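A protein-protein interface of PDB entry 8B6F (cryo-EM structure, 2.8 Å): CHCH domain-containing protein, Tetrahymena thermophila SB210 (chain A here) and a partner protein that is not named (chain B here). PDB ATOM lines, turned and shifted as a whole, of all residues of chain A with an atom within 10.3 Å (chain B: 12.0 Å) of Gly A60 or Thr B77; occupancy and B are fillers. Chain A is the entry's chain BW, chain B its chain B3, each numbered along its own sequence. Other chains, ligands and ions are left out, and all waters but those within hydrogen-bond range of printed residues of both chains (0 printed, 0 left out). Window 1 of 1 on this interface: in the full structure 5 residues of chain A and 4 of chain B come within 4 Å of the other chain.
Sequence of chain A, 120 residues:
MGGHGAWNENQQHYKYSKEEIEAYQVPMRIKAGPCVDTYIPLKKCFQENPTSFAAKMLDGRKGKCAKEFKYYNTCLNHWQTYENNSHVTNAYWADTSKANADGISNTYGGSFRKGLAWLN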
ATOM      1  N   PHE A  46      13.856  19.340   3.946  1.00  0.00           N
ATOM      2  CA  PHE A  46      13.898  20.229   2.790  1.00  0.00           C
ATOM      3  C   PHE A  46      15.077  21.189   2.875  1.00  0.00           C
ATOM      4  O   PHE A  46      15.741  21.460   1.868  1.00  0.00           O
ATOM      5  CB  PHE A  46      12.586  21.002   2.664  1.00  0.00           C
ATOM      6  CG  PHE A  46      11.535  20.273   1.883  1.00  0.00           C
ATOM      7  CD1 PHE A  46      11.657  20.123   0.512  1.00  0.00           C
ATOM      8  CD2 PHE A  46      10.423  19.747   2.513  1.00  0.00           C
ATOM      9  CE1 PHE A  46      10.693  19.455  -0.215  1.00  0.00           C
ATOM     10  CE2 PHE A  46       9.455  19.078   1.792  1.00  0.00           C
ATOM     11  CZ  PHE A  46       9.591  18.932   0.425  1.00  0.00           C
ATOM     12  N   PHE A  53      11.015  24.809  -6.884  1.00  0.00           N
ATOM     13  CA  PHE A  53       9.560  24.775  -6.776  1.00  0.00           C
ATOM     14  C   PHE A  53       8.945  23.923  -7.876  1.00  0.00           C
ATOM     15  O   PHE A  53       7.930  23.255  -7.651  1.00  0.00           O
ATOM     16  CB  PHE A  53       8.990  26.193  -6.816  1.00  0.00           C
ATOM     17  CG  PHE A  53       9.050  26.836  -8.170  1.00  0.00           C
ATOM     18  CD1 PHE A  53      10.203  27.466  -8.603  1.00  0.00           C
ATOM     19  CD2 PHE A  53       7.948  26.820  -9.005  1.00  0.00           C
ATOM     20  CE1 PHE A  53      10.258  28.060  -9.846  1.00  0.00           C
ATOM     21  CE2 PHE A  53       7.996  27.411 -10.251  1.00  0.00           C
ATOM     22  CZ  PHE A  53       9.152  28.034 -10.671  1.00  0.00           C
ATOM     23  N   ALA A  54       9.537  23.931  -9.071  1.00  0.00           N
ATOM     24  CA  ALA A  54       9.054  23.061 -10.135  1.00  0.00           C
ATOM     25  C   ALA A  54       9.168  21.597  -9.731  1.00  0.00           C
ATOM     26  O   ALA A  54       8.249  20.806  -9.970  1.00  0.00           O
ATOM     27  CB  ALA A  54       9.831  23.325 -11.424  1.00  0.00           C
ATOM     28  N   ALA A  55      10.289  21.218  -9.118  1.00  0.00           N
ATOM     29  CA  ALA A  55      10.446  19.846  -8.648  1.00  0.00           C
ATOM     30  C   ALA A  55       9.436  19.516  -7.558  1.00  0.00           C
ATOM     31  O   ALA A  55       8.871  18.416  -7.539  1.00  0.00           O
ATOM     32  CB  ALA A  55      11.870  19.624  -8.140  1.00  0.00           C
ATOM     33  N   LYS A  56       9.198  20.449  -6.633  1.00  0.00           N
ATOM     34  CA  LYS A  56       8.211  20.207  -5.586  1.00  0.00           C
ATOM     35  C   LYS A  56       6.830  19.970  -6.180  1.00  0.00           C
ATOM     36  O   LYS A  56       6.100  19.075  -5.738  1.00  0.00           O
ATOM     37  CB  LYS A  56       8.173  21.386  -4.614  1.00  0.00           C
ATOM     38  CG  LYS A  56       9.438  21.562  -3.790  1.00  0.00           C
ATOM     39  CD  LYS A  56       9.271  22.675  -2.763  1.00  0.00           C
ATOM     40  CE  LYS A  56      10.531  22.852  -1.931  1.00  0.00           C
ATOM     41  NZ  LYS A  56      10.379  23.923  -0.905  1.00  0.00           N
ATOM     42  N   MET A  57       6.449  20.766  -7.181  1.00  0.00           N
ATOM     43  CA  MET A  57       5.137  20.600  -7.796  1.00  0.00           C
ATOM     44  C   MET A  57       5.044  19.292  -8.571  1.00  0.00           C
ATOM     45  O   MET A  57       4.029  18.590  -8.494  1.00  0.00           O
ATOM     46  CB  MET A  57       4.841  21.779  -8.723  1.00  0.00           C
ATOM     47  CG  MET A  57       4.580  23.086  -7.996  1.00  0.00           C
ATOM     48  SD  MET A  57       3.935  24.367  -9.087  1.00  0.00           S
ATOM     49  CE  MET A  57       5.310  24.578 -10.213  1.00  0.00           C
ATOM     50  N   LEU A  58       6.087  18.947  -9.325  1.00  0.00           N
ATOM     51  CA  LEU A  58       6.022  17.806 -10.228  1.00  0.00           C
ATOM     52  C   LEU A  58       6.323  16.475  -9.553  1.00  0.00           C
ATOM     53  O   LEU A  58       6.066  15.428 -10.156  1.00  0.00           O
ATOM     54  CB  LEU A  58       6.993  18.010 -11.394  1.00  0.00           C
ATOM     55  CG  LEU A  58       6.731  19.220 -12.294  1.00  0.00           C
ATOM     56  CD1 LEU A  58       7.800  19.324 -13.364  1.00  0.00           C
ATOM     57  CD2 LEU A  58       5.351  19.148 -12.927  1.00  0.00           C
ATOM     58  N   ASP A  59       6.850  16.478  -8.332  1.00  0.00           N
ATOM     59  CA  ASP A  59       7.164  15.249  -7.615  1.00  0.00           C
ATOM     60  C   ASP A  59       6.010  14.924  -6.673  1.00  0.00           C
ATOM     61  O   ASP A  59       5.728  15.689  -5.746  1.00  0.00           O
ATOM     62  CB  ASP A  59       8.473  15.393  -6.839  1.00  0.00           C
ATOM     63  CG  ASP A  59       9.011  14.062  -6.353  1.00  0.00           C
ATOM     64  OD1 ASP A  59       8.208  13.122  -6.178  1.00  0.00           O
ATOM     65  OD2 ASP A  59      10.236  13.955  -6.142  1.00  0.00           O
ATOM     66  N   GLY A  60       5.352  13.788  -6.909  1.00  0.00           N
ATOM     67  CA  GLY A  60       4.209  13.399  -6.107  1.00  0.00           C
ATOM     68  C   GLY A  60       4.538  12.753  -4.780  1.00  0.00           C
ATOM     69  O   GLY A  60       3.648  12.618  -3.936  1.00  0.00           O
ATOM     70  N   ARG A  61       5.792  12.351  -4.576  1.00  0.00           N
ATOM     71  CA  ARG A  61       6.231  11.735  -3.331  1.00  0.00           C
ATOM     72  C   ARG A  61       7.238  12.597  -2.581  1.00  0.00           C
ATOM     73  O   ARG A  61       7.846  12.128  -1.614  1.00  0.00           O
ATOM     74  CB  ARG A  61       6.835  10.359  -3.612  1.00  0.00           C
ATOM     75  CG  ARG A  61       5.861   9.373  -4.235  1.00  0.00           C
ATOM     76  CD  ARG A  61       6.563   8.078  -4.608  1.00  0.00           C
ATOM     77  NE  ARG A  61       5.638   7.088  -5.144  1.00  0.00           N
ATOM     78  CZ  ARG A  61       4.972   6.204  -4.412  1.00  0.00           C
ATOM     79  NH1 ARG A  61       5.095   6.161  -3.097  1.00  0.00           N
ATOM     80  NH2 ARG A  61       4.162   5.341  -5.018  1.00  0.00           N
ATOM     81  N   LYS A  62       7.430  13.843  -3.004  1.00  0.00           N
ATOM     82  CA  LYS A  62       8.391  14.756  -2.394  1.00  0.00           C
ATOM     83  C   LYS A  62       9.813  14.207  -2.438  1.00  0.00           C
ATOM     84  O   LYS A  62      10.655  14.590  -1.621  1.00  0.00           O
ATOM     85  CB  LYS A  62       7.996  15.089  -0.951  1.00  0.00           C
ATOM     86  CG  LYS A  62       6.630  15.751  -0.825  1.00  0.00           C
ATOM     87  CD  LYS A  62       6.581  17.087  -1.556  1.00  0.00           C
ATOM     88  CE  LYS A  62       5.220  17.746  -1.426  1.00  0.00           C
ATOM     89  NZ  LYS A  62       4.152  16.971  -2.111  1.00  0.00           N
ATOM     90  N   GLY A  63      10.092  13.316  -3.387  1.00  0.00           N
ATOM     91  CA  GLY A  63      11.433  12.811  -3.601  1.00  0.00           C
ATOM     92  C   GLY A  63      12.150  12.367  -2.346  1.00  0.00           C
ATOM     93  O   GLY A  63      11.736  11.412  -1.682  1.00  0.00           O
ATOM     94  N   LYS A  64      13.239  13.062  -2.014  1.00  0.00           N
ATOM     95  CA  LYS A  64      14.074  12.645  -0.894  1.00  0.00           C
ATOM     96  C   LYS A  64      13.308  12.702   0.421  1.00  0.00           C
ATOM     97  O   LYS A  64      13.434  11.802   1.260  1.00  0.00           O
ATOM     98  CB  LYS A  64      15.325  13.519  -0.825  1.00  0.00           C
ATOM     99  CG  LYS A  64      16.155  13.498  -2.103  1.00  0.00           C
ATOM    100  CD  LYS A  64      17.345  14.440  -2.006  1.00  0.00           C
ATOM    101  CE  LYS A  64      18.126  14.488  -3.310  1.00  0.00           C
ATOM    102  NZ  LYS A  64      18.680  13.157  -3.688  1.00  0.00           N
ATOM    103  N   CYS A  65      12.512  13.746   0.621  1.00  0.00           N
ATOM    104  CA  CYS A  65      11.783  13.927   1.876  1.00  0.00           C
ATOM    105  C   CYS A  65      10.426  13.235   1.839  1.00  0.00           C
ATOM    106  O   CYS A  65       9.386  13.838   2.096  1.00  0.00           O
ATOM    107  CB  CYS A  65      11.630  15.414   2.174  1.00  0.00           C
ATOM    108  SG  CYS A  65      13.201  16.304   2.203  1.00  0.00           S
ATOM    109  N   ALA A  66      10.436  11.941   1.522  1.00  0.00           N
ATOM    110  CA  ALA A  66       9.209  11.158   1.477  1.00  0.00           C
ATOM    111  C   ALA A  66       8.888  10.522   2.821  1.00  0.00           C
ATOM    112  O   ALA A  66       7.715  10.434   3.199  1.00  0.00           O
ATOM    113  CB  ALA A  66       9.316  10.073   0.404  1.00  0.00           C
ATOM    114  N   LYS A  67       9.910  10.072   3.551  1.00  0.00           N
ATOM    115  CA  LYS A  67       9.671   9.421   4.835  1.00  0.00           C
ATOM    116  C   LYS A  67       8.973  10.367   5.801  1.00  0.00           C
ATOM    117  O   LYS A  67       8.012   9.984   6.478  1.00  0.00           O
ATOM    118  CB  LYS A  67      10.991   8.924   5.424  1.00  0.00           C
ATOM    119  CG  LYS A  67      10.842   8.256   6.787  1.00  0.00           C
ATOM    120  CD  LYS A  67      12.161   7.677   7.281  1.00  0.00           C
ATOM    121  CE  LYS A  67      13.217   8.753   7.505  1.00  0.00           C
ATOM    122  NZ  LYS A  67      12.769   9.804   8.458  1.00  0.00           N
ATOM    123  N   PHE A  69       7.398  13.175   4.831  1.00  0.00           N
ATOM    124  CA  PHE A  69       6.170  13.662   4.220  1.00  0.00           C
ATOM    125  C   PHE A  69       5.012  12.698   4.430  1.00  0.00           C
ATOM    126  O   PHE A  69       3.854  13.126   4.457  1.00  0.00           O
ATOM    127  CB  PHE A  69       6.376  13.908   2.728  1.00  0.00           C
ATOM    128  CG  PHE A  69       5.135  14.365   2.024  1.00  0.00           C
ATOM    129  CD1 PHE A  69       4.659  15.653   2.196  1.00  0.00           C
ATOM    130  CD2 PHE A  69       4.435  13.499   1.203  1.00  0.00           C
ATOM    131  CE1 PHE A  69       3.513  16.072   1.556  1.00  0.00           C
ATOM    132  CE2 PHE A  69       3.288  13.912   0.559  1.00  0.00           C
ATOM    133  CZ  PHE A  69       2.826  15.200   0.735  1.00  0.00           C
ATOM    134  N   LYS A  70       5.291  11.403   4.586  1.00  0.00           N
ATOM    135  CA  LYS A  70       4.214  10.466   4.884  1.00  0.00           C
ATOM    136  C   LYS A  70       3.542  10.825   6.201  1.00  0.00           C
ATOM    137  O   LYS A  70       2.314  10.943   6.274  1.00  0.00           O
ATOM    138  CB  LYS A  70       4.748   9.034   4.923  1.00  0.00           C
ATOM    139  CG  LYS A  70       5.096   8.465   3.554  1.00  0.00           C
ATOM    140  CD  LYS A  70       5.682   7.062   3.654  1.00  0.00           C
ATOM    141  CE  LYS A  70       4.651   6.058   4.159  1.00  0.00           C
ATOM    142  NZ  LYS A  70       5.194   4.669   4.199  1.00  0.00           N
ATOM    143  N   ASN A  73       1.730  14.190   5.835  1.00  0.00           N
ATOM    144  CA  ASN A  73       0.508  14.105   5.046  1.00  0.00           C
ATOM    145  C   ASN A  73      -0.612  13.444   5.835  1.00  0.00           C
ATOM    146  O   ASN A  73      -1.765  13.886   5.774  1.00  0.00           O
ATOM    147  CB  ASN A  73       0.779  13.341   3.752  1.00  0.00           C
ATOM    148  CG  ASN A  73      -0.393  13.385   2.795  1.00  0.00           C
ATOM    149  OD1 ASN A  73      -1.228  14.286   2.861  1.00  0.00           O
ATOM    150  ND2 ASN A  73      -0.462  12.411   1.897  1.00  0.00           N
ATOM    151  N   LEU B  67       4.593  16.749 -22.426  1.00  0.00           N
ATOM    152  CA  LEU B  67       3.909  15.797 -21.557  1.00  0.00           C
ATOM    153  C   LEU B  67       4.628  14.455 -21.533  1.00  0.00           C
ATOM    154  O   LEU B  67       4.701  13.802 -20.487  1.00  0.00           O
ATOM    155  CB  LEU B  67       2.457  15.631 -22.001  1.00  0.00           C
ATOM    156  CG  LEU B  67       1.457  16.568 -21.318  1.00  0.00           C
ATOM    157  CD1 LEU B  67       1.824  18.022 -21.515  1.00  0.00           C
ATOM    158  CD2 LEU B  67       0.064  16.311 -21.841  1.00  0.00           C
ATOM    159  N   PHE B  68       5.165  14.026 -22.677  1.00  0.00           N
ATOM    160  CA  PHE B  68       5.951  12.799 -22.708  1.00  0.00           C
ATOM    161  C   PHE B  68       7.199  12.932 -21.846  1.00  0.00           C
ATOM    162  O   PHE B  68       7.554  12.008 -21.105  1.00  0.00           O
ATOM    163  CB  PHE B  68       6.324  12.458 -24.152  1.00  0.00           C
ATOM    164  CG  PHE B  68       6.829  11.057 -24.337  1.00  0.00           C
ATOM    165  CD1 PHE B  68       5.942   9.993 -24.412  1.00  0.00           C
ATOM    166  CD2 PHE B  68       8.185  10.803 -24.462  1.00  0.00           C
ATOM    167  CE1 PHE B  68       6.400   8.701 -24.590  1.00  0.00           C
ATOM    168  CE2 PHE B  68       8.651   9.513 -24.642  1.00  0.00           C
ATOM    169  CZ  PHE B  68       7.756   8.461 -24.706  1.00  0.00           C
ATOM    170  N   ALA B  69       7.881  14.075 -21.932  1.00  0.00           N
ATOM    171  CA  ALA B  69       9.054  14.305 -21.096  1.00  0.00           C
ATOM    172  C   ALA B  69       8.691  14.275 -19.618  1.00  0.00           C
ATOM    173  O   ALA B  69       9.414  13.686 -18.806  1.00  0.00           O
ATOM    174  CB  ALA B  69       9.703  15.640 -21.458  1.00  0.00           C
ATOM    175  N   TYR B  70       7.579  14.910 -19.246  1.00  0.00           N
ATOM    176  CA  TYR B  70       7.137  14.865 -17.857  1.00  0.00           C
ATOM    177  C   TYR B  70       6.834  13.442 -17.417  1.00  0.00           C
ATOM    178  O   TYR B  70       7.224  13.027 -16.319  1.00  0.00           O
ATOM    179  CB  TYR B  70       5.901  15.741 -17.660  1.00  0.00           C
ATOM    180  CG  TYR B  70       5.136  15.387 -16.408  1.00  0.00           C
ATOM    181  CD1 TYR B  70       5.546  15.849 -15.164  1.00  0.00           C
ATOM    182  CD2 TYR B  70       4.012  14.573 -16.468  1.00  0.00           C
ATOM    183  CE1 TYR B  70       4.851  15.518 -14.017  1.00  0.00           C
ATOM    184  CE2 TYR B  70       3.312  14.237 -15.329  1.00  0.00           C
ATOM    185  CZ  TYR B  70       3.734  14.712 -14.106  1.00  0.00           C
ATOM    186  OH  TYR B  70       3.039  14.380 -12.968  1.00  0.00           O
ATOM    187  N   ASP B  71       6.142  12.673 -18.258  1.00  0.00           N
ATOM    188  CA  ASP B  71       5.789  11.311 -17.881  1.00  0.00           C
ATOM    189  C   ASP B  71       7.030  10.465 -17.631  1.00  0.00           C
ATOM    190  O   ASP B  71       7.062   9.667 -16.687  1.00  0.00           O
ATOM    191  CB  ASP B  71       4.921  10.674 -18.966  1.00  0.00           C
ATOM    192  CG  ASP B  71       3.486  11.152 -18.917  1.00  0.00           C
ATOM    193  OD1 ASP B  71       2.982  11.419 -17.808  1.00  0.00           O
ATOM    194  OD2 ASP B  71       2.858  11.261 -19.988  1.00  0.00           O
ATOM    195  N   TRP B  72       8.058  10.620 -18.455  1.00  0.00           N
ATOM    196  CA  TRP B  72       9.246   9.790 -18.336  1.00  0.00           C
ATOM    197  C   TRP B  72      10.311  10.383 -17.424  1.00  0.00           C
ATOM    198  O   TRP B  72      11.351   9.745 -17.227  1.00  0.00           O
ATOM    199  CB  TRP B  72       9.830   9.524 -19.724  1.00  0.00           C
ATOM    200  CG  TRP B  72       9.071   8.466 -20.455  1.00  0.00           C
ATOM    201  CD1 TRP B  72       8.049   8.649 -21.339  1.00  0.00           C
ATOM    202  CD2 TRP B  72       9.261   7.051 -20.347  1.00  0.00           C
ATOM    203  NE1 TRP B  72       7.596   7.435 -21.794  1.00  0.00           N
ATOM    204  CE2 TRP B  72       8.324   6.438 -21.201  1.00  0.00           C
ATOM    205  CE3 TRP B  72      10.137   6.243 -19.615  1.00  0.00           C
ATOM    206  CZ2 TRP B  72       8.237   5.056 -21.343  1.00  0.00           C
ATOM    207  CZ3 TRP B  72      10.050   4.870 -19.757  1.00  0.00           C
ATOM    208  CH2 TRP B  72       9.106   4.289 -20.614  1.00  0.00           C
ATOM    209  N   THR B  73      10.092  11.571 -16.858  1.00  0.00           N
ATOM    210  CA  THR B  73      10.998  12.124 -15.858  1.00  0.00           C
ATOM    211  C   THR B  73      10.367  12.159 -14.473  1.00  0.00           C
ATOM    212  O   THR B  73      10.920  11.587 -13.530  1.00  0.00           O
ATOM    213  CB  THR B  73      11.445  13.536 -16.267  1.00  0.00           C
ATOM    214  OG1 THR B  73      10.297  14.365 -16.487  1.00  0.00           O
ATOM    215  CG2 THR B  73      12.288  13.488 -17.532  1.00  0.00           C
ATOM    216  N   TYR B  74       9.212  12.812 -14.324  1.00  0.00           N
ATOM    217  CA  TYR B  74       8.518  12.872 -13.046  1.00  0.00           C
ATOM    218  C   TYR B  74       7.254  12.026 -13.001  1.00  0.00           C
ATOM    219  O   TYR B  74       6.658  11.895 -11.928  1.00  0.00           O
ATOM    220  CB  TYR B  74       8.153  14.326 -12.704  1.00  0.00           C
ATOM    221  CG  TYR B  74       9.326  15.164 -12.247  1.00  0.00           C
ATOM    222  CD1 TYR B  74       9.716  15.178 -10.914  1.00  0.00           C
ATOM    223  CD2 TYR B  74      10.034  15.950 -13.145  1.00  0.00           C
ATOM    224  CE1 TYR B  74      10.785  15.945 -10.489  1.00  0.00           C
ATOM    225  CE2 TYR B  74      11.105  16.721 -12.731  1.00  0.00           C
ATOM    226  CZ  TYR B  74      11.473  16.714 -11.402  1.00  0.00           C
ATOM    227  OH  TYR B  74      12.536  17.478 -10.983  1.00  0.00           O
ATOM    228  N   GLY B  75       6.830  11.453 -14.129  1.00  0.00           N
ATOM    229  CA  GLY B  75       5.633  10.635 -14.124  1.00  0.00           C
ATOM    230  C   GLY B  75       5.748   9.419 -13.231  1.00  0.00           C
ATOM    231  O   GLY B  75       4.756   8.976 -12.648  1.00  0.00           O
ATOM    232  N   PHE B  76       6.953   8.860 -13.111  1.00  0.00           N
ATOM    233  CA  PHE B  76       7.143   7.698 -12.250  1.00  0.00           C
ATOM    234  C   PHE B  76       6.793   8.020 -10.805  1.00  0.00           C
ATOM    235  O   PHE B  76       6.145   7.221 -10.120  1.00  0.00           O
ATOM    236  CB  PHE B  76       8.588   7.208 -12.341  1.00  0.00           C
ATOM    237  CG  PHE B  76       8.988   6.734 -13.708  1.00  0.00           C
ATOM    238  CD1 PHE B  76       8.793   5.417 -14.080  1.00  0.00           C
ATOM    239  CD2 PHE B  76       9.572   7.601 -14.615  1.00  0.00           C
ATOM    240  CE1 PHE B  76       9.164   4.972 -15.333  1.00  0.00           C
ATOM    241  CE2 PHE B  76       9.946   7.164 -15.870  1.00  0.00           C
ATOM    242  CZ  PHE B  76       9.741   5.846 -16.229  1.00  0.00           C
ATOM    243  N   THR B  77       7.213   9.188 -10.326  1.00  0.00           N
ATOM    244  CA  THR B  77       7.065   9.550  -8.915  1.00  0.00           C
ATOM    245  C   THR B  77       5.771  10.335  -8.685  1.00  0.00           C
ATOM    246  O   THR B  77       5.773  11.496  -8.278  1.00  0.00           O
ATOM    247  CB  THR B  77       8.283  10.337  -8.438  1.00  0.00           C
ATOM    248  OG1 THR B  77       8.057  10.813  -7.104  1.00  0.00           O
ATOM    249  CG2 THR B  77       8.574  11.528  -9.351  1.00  0.00           C
ATOM    250  N   GLN B  78       4.650   9.670  -8.950  1.00  0.00           N
ATOM    251  CA  GLN B  78       3.333  10.200  -8.630  1.00  0.00           C
ATOM    252  C   GLN B  78       2.510   9.112  -7.957  1.00  0.00           C
ATOM    253  O   GLN B  78       2.727   7.920  -8.183  1.00  0.00           O
ATOM    254  CB  GLN B  78       2.605  10.725  -9.878  1.00  0.00           C
ATOM    255  CG  GLN B  78       2.129   9.651 -10.841  1.00  0.00           C
ATOM    256  CD  GLN B  78       1.468  10.241 -12.073  1.00  0.00           C
ATOM    257  OE1 GLN B  78       1.556  11.442 -12.324  1.00  0.00           O
ATOM    258  NE2 GLN B  78       0.796   9.396 -12.846  1.00  0.00           N
ATOM    259  N   VAL B  79       1.564   9.536  -7.121  1.00  0.00           N
ATOM    260  CA  VAL B  79       0.752   8.633  -6.313  1.00  0.00           C
ATOM    261  C   VAL B  79      -0.685   8.706  -6.803  1.00  0.00           C
ATOM    262  O   VAL B  79      -1.239   9.799  -6.973  1.00  0.00           O
ATOM    263  CB  VAL B  79       0.845   8.979  -4.815  1.00  0.00           C
ATOM    264  CG1 VAL B  79       2.284   8.892  -4.341  1.00  0.00           C
ATOM    265  CG2 VAL B  79       0.277  10.364  -4.535  1.00  0.00           C
ATOM    266  N   ASP B  80      -1.283   7.543  -7.046  1.00  0.00           N
ATOM    267  CA  ASP B  80      -2.666   7.493  -7.493  1.00  0.00           C
ATOM    268  C   ASP B  80      -3.593   8.005  -6.400  1.00  0.00           C
ATOM    269  O   ASP B  80      -3.430   7.680  -5.221  1.00  0.00           O
ATOM    270  CB  ASP B  80      -3.044   6.062  -7.879  1.00  0.00           C
ATOM    271  CG  ASP B  80      -4.419   5.972  -8.510  1.00  0.00           C
ATOM    272  OD1 ASP B  80      -5.047   7.030  -8.728  1.00  0.00           O
ATOM    273  OD2 ASP B  80      -4.873   4.843  -8.788  1.00  0.00           O
ATOM    274  N   ALA B  81      -4.573   8.815  -6.796  1.00  0.00           N
ATOM    275  CA  ALA B  81      -5.558   9.385  -5.879  1.00  0.00           C
ATOM    276  C   ALA B  81      -6.945   8.994  -6.377  1.00  0.00           C
ATOM    277  O   ALA B  81      -7.481   9.622  -7.294  1.00  0.00           O
ATOM    278  CB  ALA B  81      -5.406  10.900  -5.785  1.00  0.00           C
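The side-chain carboxylate (OD1) of Asp A59 is in hydrogen-bond range of the side-chain hydroxyl (OG1) of Thr B77, 2.5 Å away.
The backbone NH (N) of Gly A60 lies within hydrogen-bond range of the backbone carbonyl oxygen (O) of Thr B77 (2.7 Å).
The side-chain carboxylate (OD1) of Asp A59 sits at hydrogen-bond distance from the backbone NH (N) of Arg A61 (3.0 Å).
The side-chain carboxylate (OD1) of Asp A59 lies within hydrogen-bond range of the backbone NH (N) of Lys A62 (3.3 Å).
OD2 of Asp A59 is in hydrogen-bond range of N of Gly A63.
O of Tyr B70 sits at hydrogen-bond distance from OG1 of Thr B73 (3.4 Å).
The side-chain hydroxyl of Tyr B70 is in hydrogen-bond range of the side-chain amide oxygen of Gln B78 (3.4 Å).
The backbone carbonyl oxygen (O) of Tyr B70 is in hydrogen-bond range of the backbone NH (N) of Gly B75, 2.7 Å away.
Among the printed residues, merely in contact across the chains: Ala A55 with Tyr B74, Leu A58 with Tyr B70, Leu A58 with Tyr B74, Gly A60 with Val B79, Arg A61 with Thr B77 and Arg A61 with Val B79.
Printed residues of chain B within 4 Å of Gly A60: Thr B77 and Val B79.
Of chain B, only Thr B77 (3.7 Å) and Val B79 (3.6 Å) come within 4 Å of Arg A61.
Gly B75 touches none of the printed residues of chain A.
Of the printed residues of chain A, Val B79 touches Gly A60 (3.99 Å) and Arg A61 (3.6 Å).
Of the printed residues of chain B, Leu A58 touches Tyr B70 and Tyr B74.
Of the printed residues of chain A, Tyr B70 touches Leu A58.
The nearest printed residue of chain B that does not touch Gly A60 is Gln B78 (4.2 Å).
The nearest residue of chain A that does not touch Thr B77 is Leu A58 (4.4 Å).
Hydrophobic or aromatic side chains of chain B within 4 Å of the printed part of chain A: Tyr B70, Tyr B74 and Val B79.
Along chain B the printed residues that touch a printed residue of chain A span positions 70 to 79.
Hydrophobic or aromatic side chains of chain A that line the printed part of chain B: Ala A55 and Leu A58.
Among the printed residues, 8 pairs touch across the chains.
Among the printed residues, no Asp or Glu carboxylate lies within 4 Å of a Lys or Arg side-chain nitrogen of the other chain.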
